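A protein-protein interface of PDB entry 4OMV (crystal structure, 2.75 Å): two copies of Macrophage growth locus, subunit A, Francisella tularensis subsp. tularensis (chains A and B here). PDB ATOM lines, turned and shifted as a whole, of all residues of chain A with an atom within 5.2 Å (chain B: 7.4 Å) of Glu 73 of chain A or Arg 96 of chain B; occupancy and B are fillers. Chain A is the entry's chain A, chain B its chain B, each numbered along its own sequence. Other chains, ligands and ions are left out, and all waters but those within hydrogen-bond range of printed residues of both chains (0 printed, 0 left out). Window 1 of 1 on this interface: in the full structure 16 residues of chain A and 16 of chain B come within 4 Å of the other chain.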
ATOM      1  N   LEU A  68      -1.612  22.462 -20.767  1.00  0.00           N
ATOM      2  CA  LEU A  68      -1.319  21.619 -21.936  1.00  0.00           C
ATOM      3  C   LEU A  68      -0.042  22.019 -22.720  1.00  0.00           C
ATOM      4  O   LEU A  68       0.780  21.144 -23.007  1.00  0.00           O
ATOM      5  CB  LEU A  68      -2.521  21.576 -22.901  1.00  0.00           C
ATOM      6  CG  LEU A  68      -2.301  20.756 -24.185  1.00  0.00           C
ATOM      7  CD1 LEU A  68      -2.488  19.261 -23.955  1.00  0.00           C
ATOM      8  CD2 LEU A  68      -3.153  21.259 -25.300  1.00  0.00           C
ATOM      9  N   SER A  69       0.100  23.304 -23.091  1.00  0.00           N
ATOM     10  CA  SER A  69       1.241  23.750 -23.884  1.00  0.00           C
ATOM     11  C   SER A  69       2.571  23.587 -23.120  1.00  0.00           C
ATOM     12  O   SER A  69       3.600  23.256 -23.719  1.00  0.00           O
ATOM     13  CB  SER A  69       1.039  25.188 -24.342  1.00  0.00           C
ATOM     14  OG  SER A  69       1.256  26.109 -23.288  1.00  0.00           O
ATOM     15  N   VAL A  70       2.517  23.776 -21.791  1.00  0.00           N
ATOM     16  CA  VAL A  70       3.653  23.648 -20.871  1.00  0.00           C
ATOM     17  C   VAL A  70       3.957  22.148 -20.693  1.00  0.00           C
ATOM     18  O   VAL A  70       5.128  21.772 -20.673  1.00  0.00           O
ATOM     19  CB  VAL A  70       3.384  24.394 -19.537  1.00  0.00           C
ATOM     20  CG1 VAL A  70       4.600  24.350 -18.608  1.00  0.00           C
ATOM     21  CG2 VAL A  70       2.964  25.837 -19.812  1.00  0.00           C
ATOM     22  N   ILE A  71       2.914  21.291 -20.678  1.00  0.00           N
ATOM     23  CA  ILE A  71       3.091  19.842 -20.615  1.00  0.00           C
ATOM     24  C   ILE A  71       3.839  19.400 -21.896  1.00  0.00           C
ATOM     25  O   ILE A  71       4.848  18.700 -21.786  1.00  0.00           O
ATOM     26  CB  ILE A  71       1.748  19.068 -20.407  1.00  0.00           C
ATOM     27  CG1 ILE A  71       1.135  19.319 -19.017  1.00  0.00           C
ATOM     28  CG2 ILE A  71       1.964  17.579 -20.592  1.00  0.00           C
ATOM     29  CD1 ILE A  71      -0.327  18.933 -18.908  1.00  0.00           C
ATOM     30  N   ILE A  72       3.384  19.858 -23.091  1.00  0.00           N
ATOM     31  CA  ILE A  72       3.977  19.475 -24.376  1.00  0.00           C
ATOM     32  C   ILE A  72       5.453  19.928 -24.460  1.00  0.00           C
ATOM     33  O   ILE A  72       6.300  19.149 -24.902  1.00  0.00           O
ATOM     34  CB  ILE A  72       3.118  19.961 -25.588  1.00  0.00           C
ATOM     35  CG1 ILE A  72       1.696  19.296 -25.573  1.00  0.00           C
ATOM     36  CG2 ILE A  72       3.807  19.671 -26.923  1.00  0.00           C
ATOM     37  CD1 ILE A  72       0.606  19.977 -26.514  1.00  0.00           C
ATOM     38  N   GLU A  73       5.768  21.140 -23.978  1.00  0.00           N
ATOM     39  CA  GLU A  73       7.130  21.676 -23.991  1.00  0.00           C
ATOM     40  C   GLU A  73       8.057  20.912 -23.049  1.00  0.00           C
ATOM     41  O   GLU A  73       9.181  20.594 -23.439  1.00  0.00           O
ATOM     42  CB  GLU A  73       7.129  23.170 -23.637  1.00  0.00           C
ATOM     43  CG  GLU A  73       6.586  24.093 -24.717  1.00  0.00           C
ATOM     44  CD  GLU A  73       7.177  23.998 -26.106  1.00  0.00           C
ATOM     45  OE1 GLU A  73       8.392  23.726 -26.270  1.00  0.00           O
ATOM     46  OE2 GLU A  73       6.399  24.276 -27.042  1.00  0.00           O
ATOM     47  N   ALA A  74       7.570  20.576 -21.833  1.00  0.00           N
ATOM     48  CA  ALA A  74       8.313  19.808 -20.836  1.00  0.00           C
ATOM     49  C   ALA A  74       8.634  18.395 -21.357  1.00  0.00           C
ATOM     50  O   ALA A  74       9.751  17.924 -21.139  1.00  0.00           O
ATOM     51  CB  ALA A  74       7.528  19.720 -19.535  1.00  0.00           C
ATOM     52  N   ILE A  75       7.678  17.739 -22.065  1.00  0.00           N
ATOM     53  CA  ILE A  75       7.882  16.406 -22.620  1.00  0.00           C
ATOM     54  C   ILE A  75       8.962  16.488 -23.720  1.00  0.00           C
ATOM     55  O   ILE A  75       9.851  15.632 -23.762  1.00  0.00           O
ATOM     56  CB  ILE A  75       6.561  15.773 -23.126  1.00  0.00           C
ATOM     57  CG1 ILE A  75       5.635  15.386 -21.935  1.00  0.00           C
ATOM     58  CG2 ILE A  75       6.832  14.560 -24.026  1.00  0.00           C
ATOM     59  CD1 ILE A  75       4.152  15.225 -22.309  1.00  0.00           C
ATOM     60  N   GLU A  76       8.902  17.534 -24.571  1.00  0.00           N
ATOM     61  CA  GLU A  76       9.861  17.753 -25.665  1.00  0.00           C
ATOM     62  C   GLU A  76      11.274  18.039 -25.147  1.00  0.00           C
ATOM     63  O   GLU A  76      12.239  17.557 -25.734  1.00  0.00           O
ATOM     64  CB  GLU A  76       9.392  18.893 -26.576  1.00  0.00           C
ATOM     65  CG  GLU A  76       8.244  18.490 -27.478  1.00  0.00           C
ATOM     66  CD  GLU A  76       8.615  18.371 -28.946  1.00  0.00           C
ATOM     67  OE1 GLU A  76       8.739  19.415 -29.622  1.00  0.00           O
ATOM     68  OE2 GLU A  76       8.789  17.229 -29.421  1.00  0.00           O
ATOM     69  N   ASP A  77      11.393  18.797 -24.054  1.00  0.00           N
ATOM     70  CA  ASP A  77      12.678  19.101 -23.431  1.00  0.00           C
ATOM     71  C   ASP A  77      13.355  17.810 -22.937  1.00  0.00           C
ATOM     72  O   ASP A  77      14.549  17.633 -23.138  1.00  0.00           O
ATOM     73  CB  ASP A  77      12.506  20.095 -22.250  1.00  0.00           C
ATOM     74  CG  ASP A  77      12.135  21.533 -22.607  1.00  0.00           C
ATOM     75  OD1 ASP A  77      12.490  21.987 -23.720  1.00  0.00           O
ATOM     76  OD2 ASP A  77      11.538  22.222 -21.751  1.00  0.00           O
ATOM     77  N   LEU A  78      12.579  16.899 -22.325  1.00  0.00           N
ATOM     78  CA  LEU A  78      13.085  15.661 -21.742  1.00  0.00           C
ATOM     79  C   LEU A  78      13.180  14.522 -22.750  1.00  0.00           C
ATOM     80  O   LEU A  78      14.119  13.726 -22.668  1.00  0.00           O
ATOM     81  CB  LEU A  78      12.213  15.243 -20.548  1.00  0.00           C
ATOM     82  CG  LEU A  78      12.135  16.255 -19.395  1.00  0.00           C
ATOM     83  CD1 LEU A  78      10.945  15.995 -18.554  1.00  0.00           C
ATOM     84  CD2 LEU A  78      13.388  16.270 -18.560  1.00  0.00           C
ATOM     85  N   PHE A  85       7.288  19.249 -33.045  1.00  0.00           N
ATOM     86  CA  PHE A  85       7.250  20.612 -33.607  1.00  0.00           C
ATOM     87  C   PHE A  85       8.073  20.780 -34.889  1.00  0.00           C
ATOM     88  O   PHE A  85       9.074  20.056 -35.028  1.00  0.00           O
ATOM     89  CB  PHE A  85       7.790  21.629 -32.569  1.00  0.00           C
ATOM     90  CG  PHE A  85       6.790  22.028 -31.511  1.00  0.00           C
ATOM     91  CD1 PHE A  85       5.726  22.867 -31.818  1.00  0.00           C
ATOM     92  CD2 PHE A  85       6.908  21.560 -30.210  1.00  0.00           C
ATOM     93  CE1 PHE A  85       4.782  23.205 -30.847  1.00  0.00           C
ATOM     94  CE2 PHE A  85       5.962  21.891 -29.238  1.00  0.00           C
ATOM     95  CZ  PHE A  85       4.913  22.727 -29.559  1.00  0.00           C
ATOM     96  N   ARG A  96       2.945  26.976 -32.496  1.00  0.00           N
ATOM     97  CA  ARG A  96       2.626  27.281 -31.106  1.00  0.00           C
ATOM     98  C   ARG A  96       1.417  28.215 -30.985  1.00  0.00           C
ATOM     99  O   ARG A  96       0.616  28.066 -30.056  1.00  0.00           O
ATOM    100  CB  ARG A  96       3.848  27.875 -30.412  1.00  0.00           C
ATOM    101  CG  ARG A  96       4.896  26.840 -30.138  1.00  0.00           C
ATOM    102  CD  ARG A  96       6.138  27.512 -29.601  1.00  0.00           C
ATOM    103  NE  ARG A  96       7.037  26.508 -29.063  1.00  0.00           N
ATOM    104  CZ  ARG A  96       8.347  26.472 -29.273  1.00  0.00           C
ATOM    105  NH1 ARG A  96       8.933  27.409 -30.007  1.00  0.00           N
ATOM    106  NH2 ARG A  96       9.085  25.506 -28.739  1.00  0.00           N
ATOM    107  N   SER B  69       5.967  33.254 -23.581  1.00  0.00           N
ATOM    108  CA  SER B  69       6.759  32.049 -23.762  1.00  0.00           C
ATOM    109  C   SER B  69       7.098  31.829 -25.249  1.00  0.00           C
ATOM    110  O   SER B  69       8.206  31.381 -25.563  1.00  0.00           O
ATOM    111  CB  SER B  69       6.045  30.838 -23.176  1.00  0.00           C
ATOM    112  OG  SER B  69       4.977  30.401 -24.000  1.00  0.00           O
ATOM    113  N   VAL B  70       6.165  32.193 -26.156  1.00  0.00           N
ATOM    114  CA  VAL B  70       6.329  32.062 -27.609  1.00  0.00           C
ATOM    115  C   VAL B  70       7.278  33.177 -28.114  1.00  0.00           C
ATOM    116  O   VAL B  70       8.162  32.896 -28.924  1.00  0.00           O
ATOM    117  CB  VAL B  70       4.949  32.056 -28.339  1.00  0.00           C
ATOM    118  CG1 VAL B  70       5.101  31.773 -29.835  1.00  0.00           C
ATOM    119  CG2 VAL B  70       4.007  31.024 -27.708  1.00  0.00           C
ATOM    120  N   GLU B  73      10.806  32.064 -27.005  1.00  0.00           N
ATOM    121  CA  GLU B  73      11.279  30.959 -27.850  1.00  0.00           C
ATOM    122  C   GLU B  73      11.703  31.431 -29.234  1.00  0.00           C
ATOM    123  O   GLU B  73      12.773  31.041 -29.681  1.00  0.00           O
ATOM    124  CB  GLU B  73      10.246  29.828 -27.952  1.00  0.00           C
ATOM    125  CG  GLU B  73      10.085  29.012 -26.664  1.00  0.00           C
ATOM    126  CD  GLU B  73      11.338  28.428 -26.024  1.00  0.00           C
ATOM    127  OE1 GLU B  73      12.156  27.855 -26.776  1.00  0.00           O
ATOM    128  OE2 GLU B  73      11.490  28.504 -24.781  1.00  0.00           O
ATOM    129  N   GLU B  76      15.003  33.313 -28.880  1.00  0.00           N
ATOM    130  CA  GLU B  76      16.045  32.313 -28.607  1.00  0.00           C
ATOM    131  C   GLU B  76      16.428  31.547 -29.864  1.00  0.00           C
ATOM    132  O   GLU B  76      17.610  31.276 -30.057  1.00  0.00           O
ATOM    133  CB  GLU B  76      15.622  31.347 -27.506  1.00  0.00           C
ATOM    134  CG  GLU B  76      15.609  31.992 -26.132  1.00  0.00           C
ATOM    135  CD  GLU B  76      16.654  31.467 -25.182  1.00  0.00           C
ATOM    136  OE1 GLU B  76      16.426  30.391 -24.582  1.00  0.00           O
ATOM    137  OE2 GLU B  76      17.682  32.158 -25.003  1.00  0.00           O
ATOM    138  N   PHE B  85      17.719  30.239 -20.792  1.00  0.00           N
ATOM    139  CA  PHE B  85      17.390  29.009 -20.081  1.00  0.00           C
ATOM    140  C   PHE B  85      18.617  28.092 -19.966  1.00  0.00           C
ATOM    141  O   PHE B  85      19.579  28.206 -20.741  1.00  0.00           O
ATOM    142  CB  PHE B  85      16.268  28.234 -20.826  1.00  0.00           C
ATOM    143  CG  PHE B  85      14.921  28.897 -20.872  1.00  0.00           C
ATOM    144  CD1 PHE B  85      14.102  28.936 -19.738  1.00  0.00           C
ATOM    145  CD2 PHE B  85      14.450  29.469 -22.048  1.00  0.00           C
ATOM    146  CE1 PHE B  85      12.844  29.549 -19.779  1.00  0.00           C
ATOM    147  CE2 PHE B  85      13.194  30.079 -22.089  1.00  0.00           C
ATOM    148  CZ  PHE B  85      12.403  30.118 -20.951  1.00  0.00           C
ATOM    149  N   PRO B  86      18.567  27.133 -19.019  1.00  0.00           N
ATOM    150  CA  PRO B  86      19.645  26.153 -18.916  1.00  0.00           C
ATOM    151  C   PRO B  86      19.714  25.359 -20.200  1.00  0.00           C
ATOM    152  O   PRO B  86      18.726  25.155 -20.898  1.00  0.00           O
ATOM    153  CB  PRO B  86      19.245  25.301 -17.708  1.00  0.00           C
ATOM    154  CG  PRO B  86      18.251  26.102 -16.964  1.00  0.00           C
ATOM    155  CD  PRO B  86      17.526  26.866 -18.012  1.00  0.00           C
ATOM    156  N   PRO B  89      18.680  19.337 -20.655  1.00  0.00           N
ATOM    157  CA  PRO B  89      17.233  19.036 -20.665  1.00  0.00           C
ATOM    158  C   PRO B  89      16.462  19.153 -19.344  1.00  0.00           C
ATOM    159  O   PRO B  89      15.443  19.836 -19.329  1.00  0.00           O
ATOM    160  CB  PRO B  89      17.177  17.588 -21.195  1.00  0.00           C
ATOM    161  CG  PRO B  89      18.595  17.104 -21.238  1.00  0.00           C
ATOM    162  CD  PRO B  89      19.409  18.331 -21.452  1.00  0.00           C
ATOM    163  N   LYS B  90      16.890  18.461 -18.276  1.00  0.00           N
ATOM    164  CA  LYS B  90      16.173  18.447 -16.999  1.00  0.00           C
ATOM    165  C   LYS B  90      15.979  19.876 -16.459  1.00  0.00           C
ATOM    166  O   LYS B  90      14.854  20.272 -16.149  1.00  0.00           O
ATOM    167  CB  LYS B  90      16.913  17.552 -15.980  1.00  0.00           C
ATOM    168  CG  LYS B  90      16.349  17.595 -14.565  1.00  0.00           C
ATOM    169  CD  LYS B  90      17.318  16.983 -13.569  1.00  0.00           C
ATOM    170  CE  LYS B  90      16.902  17.270 -12.143  1.00  0.00           C
ATOM    171  NZ  LYS B  90      17.690  16.477 -11.166  1.00  0.00           N
ATOM    172  N   GLN B  91      17.071  20.643 -16.416  1.00  0.00           N
ATOM    173  CA  GLN B  91      17.128  22.010 -15.906  1.00  0.00           C
ATOM    174  C   GLN B  91      16.288  22.957 -16.778  1.00  0.00           C
ATOM    175  O   GLN B  91      15.589  23.829 -16.237  1.00  0.00           O
ATOM    176  CB  GLN B  91      18.594  22.484 -15.827  1.00  0.00           C
ATOM    177  CG  GLN B  91      19.444  21.769 -14.771  1.00  0.00           C
ATOM    178  CD  GLN B  91      19.783  20.321 -15.108  1.00  0.00           C
ATOM    179  OE1 GLN B  91      19.884  19.913 -16.280  1.00  0.00           O
ATOM    180  NE2 GLN B  91      19.929  19.503 -14.067  1.00  0.00           N
ATOM    181  N   ARG B  92      16.354  22.770 -18.131  1.00  0.00           N
ATOM    182  CA  ARG B  92      15.577  23.543 -19.103  1.00  0.00           C
ATOM    183  C   ARG B  92      14.074  23.350 -18.852  1.00  0.00           C
ATOM    184  O   ARG B  92      13.340  24.334 -18.752  1.00  0.00           O
ATOM    185  CB  ARG B  92      15.936  23.152 -20.547  1.00  0.00           C
ATOM    186  CG  ARG B  92      15.492  24.202 -21.542  1.00  0.00           C
ATOM    187  CD  ARG B  92      15.650  23.751 -22.967  1.00  0.00           C
ATOM    188  NE  ARG B  92      14.474  24.076 -23.777  1.00  0.00           N
ATOM    189  CZ  ARG B  92      14.298  25.225 -24.424  1.00  0.00           C
ATOM    190  NH1 ARG B  92      15.221  26.176 -24.365  1.00  0.00           N
ATOM    191  NH2 ARG B  92      13.197  25.431 -25.136  1.00  0.00           N
ATOM    192  N   ALA B  93      13.638  22.079 -18.708  1.00  0.00           N
ATOM    193  CA  ALA B  93      12.259  21.697 -18.449  1.00  0.00           C
ATOM    194  C   ALA B  93      11.768  22.364 -17.173  1.00  0.00           C
ATOM    195  O   ALA B  93      10.749  23.033 -17.222  1.00  0.00           O
ATOM    196  CB  ALA B  93      12.145  20.182 -18.347  1.00  0.00           C
ATOM    197  N   ASN B  94      12.539  22.258 -16.066  1.00  0.00           N
ATOM    198  CA  ASN B  94      12.237  22.866 -14.773  1.00  0.00           C
ATOM    199  C   ASN B  94      12.098  24.390 -14.863  1.00  0.00           C
ATOM    200  O   ASN B  94      11.199  24.958 -14.240  1.00  0.00           O
ATOM    201  CB  ASN B  94      13.330  22.513 -13.751  1.00  0.00           C
ATOM    202  CG  ASN B  94      13.277  21.107 -13.224  1.00  0.00           C
ATOM    203  OD1 ASN B  94      12.208  20.533 -13.032  1.00  0.00           O
ATOM    204  ND2 ASN B  94      14.442  20.534 -12.937  1.00  0.00           N
ATOM    205  N   ALA B  95      12.981  25.056 -15.628  1.00  0.00           N
ATOM    206  CA  ALA B  95      12.960  26.513 -15.777  1.00  0.00           C
ATOM    207  C   ALA B  95      11.706  26.977 -16.523  1.00  0.00           C
ATOM    208  O   ALA B  95      11.068  27.956 -16.131  1.00  0.00           O
ATOM    209  CB  ALA B  95      14.207  26.989 -16.493  1.00  0.00           C
ATOM    210  N   ARG B  96      11.322  26.242 -17.567  1.00  0.00           N
ATOM    211  CA  ARG B  96      10.147  26.572 -18.376  1.00  0.00           C
ATOM    212  C   ARG B  96       8.840  26.389 -17.599  1.00  0.00           C
ATOM    213  O   ARG B  96       7.896  27.154 -17.808  1.00  0.00           O
ATOM    214  CB  ARG B  96      10.148  25.747 -19.653  1.00  0.00           C
ATOM    215  CG  ARG B  96      11.237  26.275 -20.607  1.00  0.00           C
ATOM    216  CD  ARG B  96      11.519  25.421 -21.809  1.00  0.00           C
ATOM    217  NE  ARG B  96      10.807  25.925 -22.975  1.00  0.00           N
ATOM    218  CZ  ARG B  96      10.234  25.152 -23.879  1.00  0.00           C
ATOM    219  NH1 ARG B  96      10.346  23.833 -23.801  1.00  0.00           N
ATOM    220  NH2 ARG B  96       9.572  25.689 -24.889  1.00  0.00           N
ATOM    221  N   ILE B  97       8.813  25.417 -16.674  1.00  0.00           N
ATOM    222  CA  ILE B  97       7.692  25.117 -15.790  1.00  0.00           C
ATOM    223  C   ILE B  97       7.610  26.241 -14.732  1.00  0.00           C
ATOM    224  O   ILE B  97       6.524  26.752 -14.454  1.00  0.00           O
ATOM    225  CB  ILE B  97       7.870  23.700 -15.197  1.00  0.00           C
ATOM    226  CG1 ILE B  97       7.395  22.646 -16.222  1.00  0.00           C
ATOM    227  CG2 ILE B  97       7.184  23.525 -13.835  1.00  0.00           C
ATOM    228  CD1 ILE B  97       8.097  21.433 -16.245  1.00  0.00           C
ATOM    229  N   LEU B  98       8.764  26.642 -14.174  1.00  0.00           N
ATOM    230  CA  LEU B  98       8.860  27.713 -13.189  1.00  0.00           C
ATOM    231  C   LEU B  98       8.482  29.063 -13.834  1.00  0.00           C
ATOM    232  O   LEU B  98       7.865  29.890 -13.160  1.00  0.00           O
ATOM    233  CB  LEU B  98      10.278  27.744 -12.602  1.00  0.00           C
ATOM    234  CG  LEU B  98      10.532  28.612 -11.372  1.00  0.00           C
ATOM    235  CD1 LEU B  98       9.617  28.233 -10.213  1.00  0.00           C
ATOM    236  CD2 LEU B  98      11.975  28.486 -10.941  1.00  0.00           C
ATOM    237  N   LEU B  99       8.799  29.259 -15.144  1.00  0.00           N
ATOM    238  CA  LEU B  99       8.418  30.451 -15.907  1.00  0.00           C
ATOM    239  C   LEU B  99       6.881  30.524 -16.008  1.00  0.00           C
ATOM    240  O   LEU B  99       6.305  31.602 -15.852  1.00  0.00           O
ATOM    241  CB  LEU B  99       9.074  30.451 -17.318  1.00  0.00           C
ATOM    242  CG  LEU B  99       8.495  31.397 -18.426  1.00  0.00           C
ATOM    243  CD1 LEU B  99       8.569  32.826 -18.022  1.00  0.00           C
ATOM    244  CD2 LEU B  99       9.228  31.265 -19.715  1.00  0.00           C
ATOM    245  N   GLU B 100       6.231  29.376 -16.220  1.00  0.00           N
ATOM    246  CA  GLU B 100       4.778  29.269 -16.297  1.00  0.00           C
ATOM    247  C   GLU B 100       4.148  29.623 -14.949  1.00  0.00           C
ATOM    248  O   GLU B 100       3.129  30.327 -14.914  1.00  0.00           O
ATOM    249  CB  GLU B 100       4.353  27.862 -16.756  1.00  0.00           C
ATOM    250  CG  GLU B 100       2.862  27.629 -16.783  1.00  0.00           C
ATOM    251  CD  GLU B 100       1.980  28.618 -17.531  1.00  0.00           C
ATOM    252  OE1 GLU B 100       2.430  29.231 -18.529  1.00  0.00           O
ATOM    253  OE2 GLU B 100       0.800  28.732 -17.133  1.00  0.00           O
ATOM    254  N   TYR B 101       4.785  29.184 -13.847  1.00  0.00           N
ATOM    255  CA  TYR B 101       4.310  29.470 -12.503  1.00  0.00           C
ATOM    256  C   TYR B 101       4.374  30.979 -12.250  1.00  0.00           C
ATOM    257  O   TYR B 101       3.401  31.550 -11.763  1.00  0.00           O
ATOM    258  CB  TYR B 101       5.102  28.672 -11.445  1.00  0.00           C
ATOM    259  CG  TYR B 101       4.684  29.003 -10.031  1.00  0.00           C
ATOM    260  CD1 TYR B 101       3.558  28.415  -9.461  1.00  0.00           C
ATOM    261  CD2 TYR B 101       5.371  29.958  -9.284  1.00  0.00           C
ATOM    262  CE1 TYR B 101       3.146  28.745  -8.172  1.00  0.00           C
ATOM    263  CE2 TYR B 101       4.955  30.310  -8.003  1.00  0.00           C
ATOM    264  CZ  TYR B 101       3.846  29.696  -7.449  1.00  0.00           C
ATOM    265  OH  TYR B 101       3.448  30.039  -6.182  1.00  0.00           O
ATOM    266  N   VAL B 102       5.492  31.619 -12.613  1.00  0.00           N
ATOM    267  CA  VAL B 102       5.684  33.067 -12.433  1.00  0.00           C
ATOM    268  C   VAL B 102       4.674  33.831 -13.326  1.00  0.00           C
ATOM    269  O   VAL B 102       4.113  34.852 -12.908  1.00  0.00           O
ATOM    270  CB  VAL B 102       7.163  33.503 -12.696  1.00  0.00           C
ATOM    271  CG1 VAL B 102       7.327  35.017 -12.586  1.00  0.00           C
ATOM    272  CG2 VAL B 102       8.139  32.784 -11.752  1.00  0.00           C
ATOM    273  N   GLU B 144      17.613  27.326  -8.105  1.00  0.00           N
ATOM    274  CA  GLU B 144      17.890  26.654  -9.377  1.00  0.00           C
ATOM    275  C   GLU B 144      19.306  26.989  -9.849  1.00  0.00           C
ATOM    276  O   GLU B 144      19.993  26.108 -10.372  1.00  0.00           O
ATOM    277  CB  GLU B 144      16.857  27.035 -10.452  1.00  0.00           C
ATOM    278  CG  GLU B 144      15.422  26.632 -10.136  1.00  0.00           C
ATOM    279  CD  GLU B 144      15.017  25.193 -10.395  1.00  0.00           C
ATOM    280  OE1 GLU B 144      15.631  24.276  -9.799  1.00  0.00           O
ATOM    281  OE2 GLU B 144      14.029  24.988 -11.137  1.00  0.00           O
ATOM    282  N   VAL B 160      16.440  34.115 -17.945  1.00  0.00           N
ATOM    283  CA  VAL B 160      15.117  34.697 -18.138  1.00  0.00           C
ATOM    284  C   VAL B 160      14.307  34.769 -16.815  1.00  0.00           C
ATOM    285  O   VAL B 160      13.611  35.760 -16.617  1.00  0.00           O
ATOM    286  CB  VAL B 160      14.336  33.989 -19.278  1.00  0.00           C
ATOM    287  CG1 VAL B 160      13.669  32.699 -18.827  1.00  0.00           C
ATOM    288  CG2 VAL B 160      13.339  34.924 -19.937  1.00  0.00           C
ATOM    289  N   LEU B 161      14.443  33.780 -15.900  1.00  0.00           N
ATOM    290  CA  LEU B 161      13.724  33.771 -14.618  1.00  0.00           C
ATOM    291  C   LEU B 161      14.166  34.911 -13.700  1.00  0.00           C
ATOM    292  O   LEU B 161      13.312  35.566 -13.118  1.00  0.00           O
ATOM    293  CB  LEU B 161      13.871  32.409 -13.902  1.00  0.00           C
ATOM    294  CG  LEU B 161      13.086  31.245 -14.536  1.00  0.00           C
ATOM    295  CD1 LEU B 161      13.542  29.934 -13.999  1.00  0.00           C
ATOM    296  CD2 LEU B 161      11.582  31.401 -14.308  1.00  0.00           C
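OD1 of Asp 77 of chain A lies within salt-bridge range of NE of Arg 92 of chain B, at 2.9 Å. NH1 of Arg 96 of chain B is in salt-bridge range of OD1 of Asp 77 of chain A (2.8 Å). OE1 of Glu 73 of chain A lies within salt-bridge range of NH2 of Arg 96 of chain B, 2.7 Å away.
OE1 of Glu 73 of chain B lies within salt-bridge range of NH2 of Arg 92 of chain B (3.1 Å). NE of Arg 96 of chain A is in salt-bridge range of OE2 of Glu 73 of chain A. The side-chain amide nitrogen of Asn 94 of chain B sits at hydrogen-bond distance from the backbone carbonyl oxygen of Lys 90 of chain B, 3.2 Å away. OE2 of Glu 73 of chain B is in salt-bridge range of NE of Arg 96 of chain B, at 3.2 Å.
Glu 100 of chain B touches Val 70 of chain A (CG to CG2, 3.5 Å). Ala 74 of chain A touches Ile 97 of chain B. O of Asp 77 of chain A touches CB of Pro 89 of chain B, at 3.3 Å. Asp 77 of chain A touches Ala 93 of chain B. CA of Lys 90 of chain B touches CD2 of Leu 78 of chain A, at 3.9 Å. Arg 96 of chain A touches Glu 73 of chain B. NH2 of Arg 96 of chain B touches NH2 of Arg 96 of chain A, at 3.9 Å.
Glu 73 of chain A touches just one residue of chain B: Arg 96. Of the printed residues of chain B, Arg 96 of chain A touches Glu 73 (3.4 Å) and Arg 96 (3.9 Å). Of the printed residues of chain A, Glu 73 of chain B touches Arg 96 (3.4 Å). Of the printed residues of chain A, Arg 92 of chain B touches Asp 77 (2.9 Å). Of the printed residues of chain A, Arg 96 of chain B touches Glu 73, Asp 77 and Arg 96. Printed residues of chain A within 4 Å of Glu 100 of chain B: Val 70 (3.5 Å). The nearest residue of chain B that does not touch Glu 73 of chain A is Arg 92 of chain B (5.2 Å). The nearest residue of chain A that does not touch Arg 96 of chain B is Val 70 of chain A (4.4 Å). The nearest printed residue of chain A that does not touch Pro 89 of chain B is Leu 78 of chain A (4.2 Å).
Printed residues of chain B that touch a printed residue of chain A: Glu 73, Pro 89, Lys 90, Arg 92, Ala 93, Arg 96, Ile 97 and Glu 100. Hydrophobic or aromatic side chains of chain B within 4 Å of the printed part of chain A: Pro 89, Ala 93 and Ile 97. Among the printed residues, Asp or Glu carboxylates within 4 Å of a Lys or Arg side-chain nitrogen of the other chain: Glu 73 of chain A with Arg 96 of chain B, Asp 77 of chain A with Arg 92 of chain B and Asp 77 of chain A with Arg 96 of chain B.
Glu 73 of chain A touches Arg 96 of chain B, and with the chains exchanged Arg 96 of chain A touches Glu 73 of chain B. Arg 96 of chain A touches its own counterpart, Arg 96 of chain B. 6 positions are printed for both chains. Of the 10 pairs that touch across the chains among the printed residues, 3 have their exchanged pair printed and touching as well.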
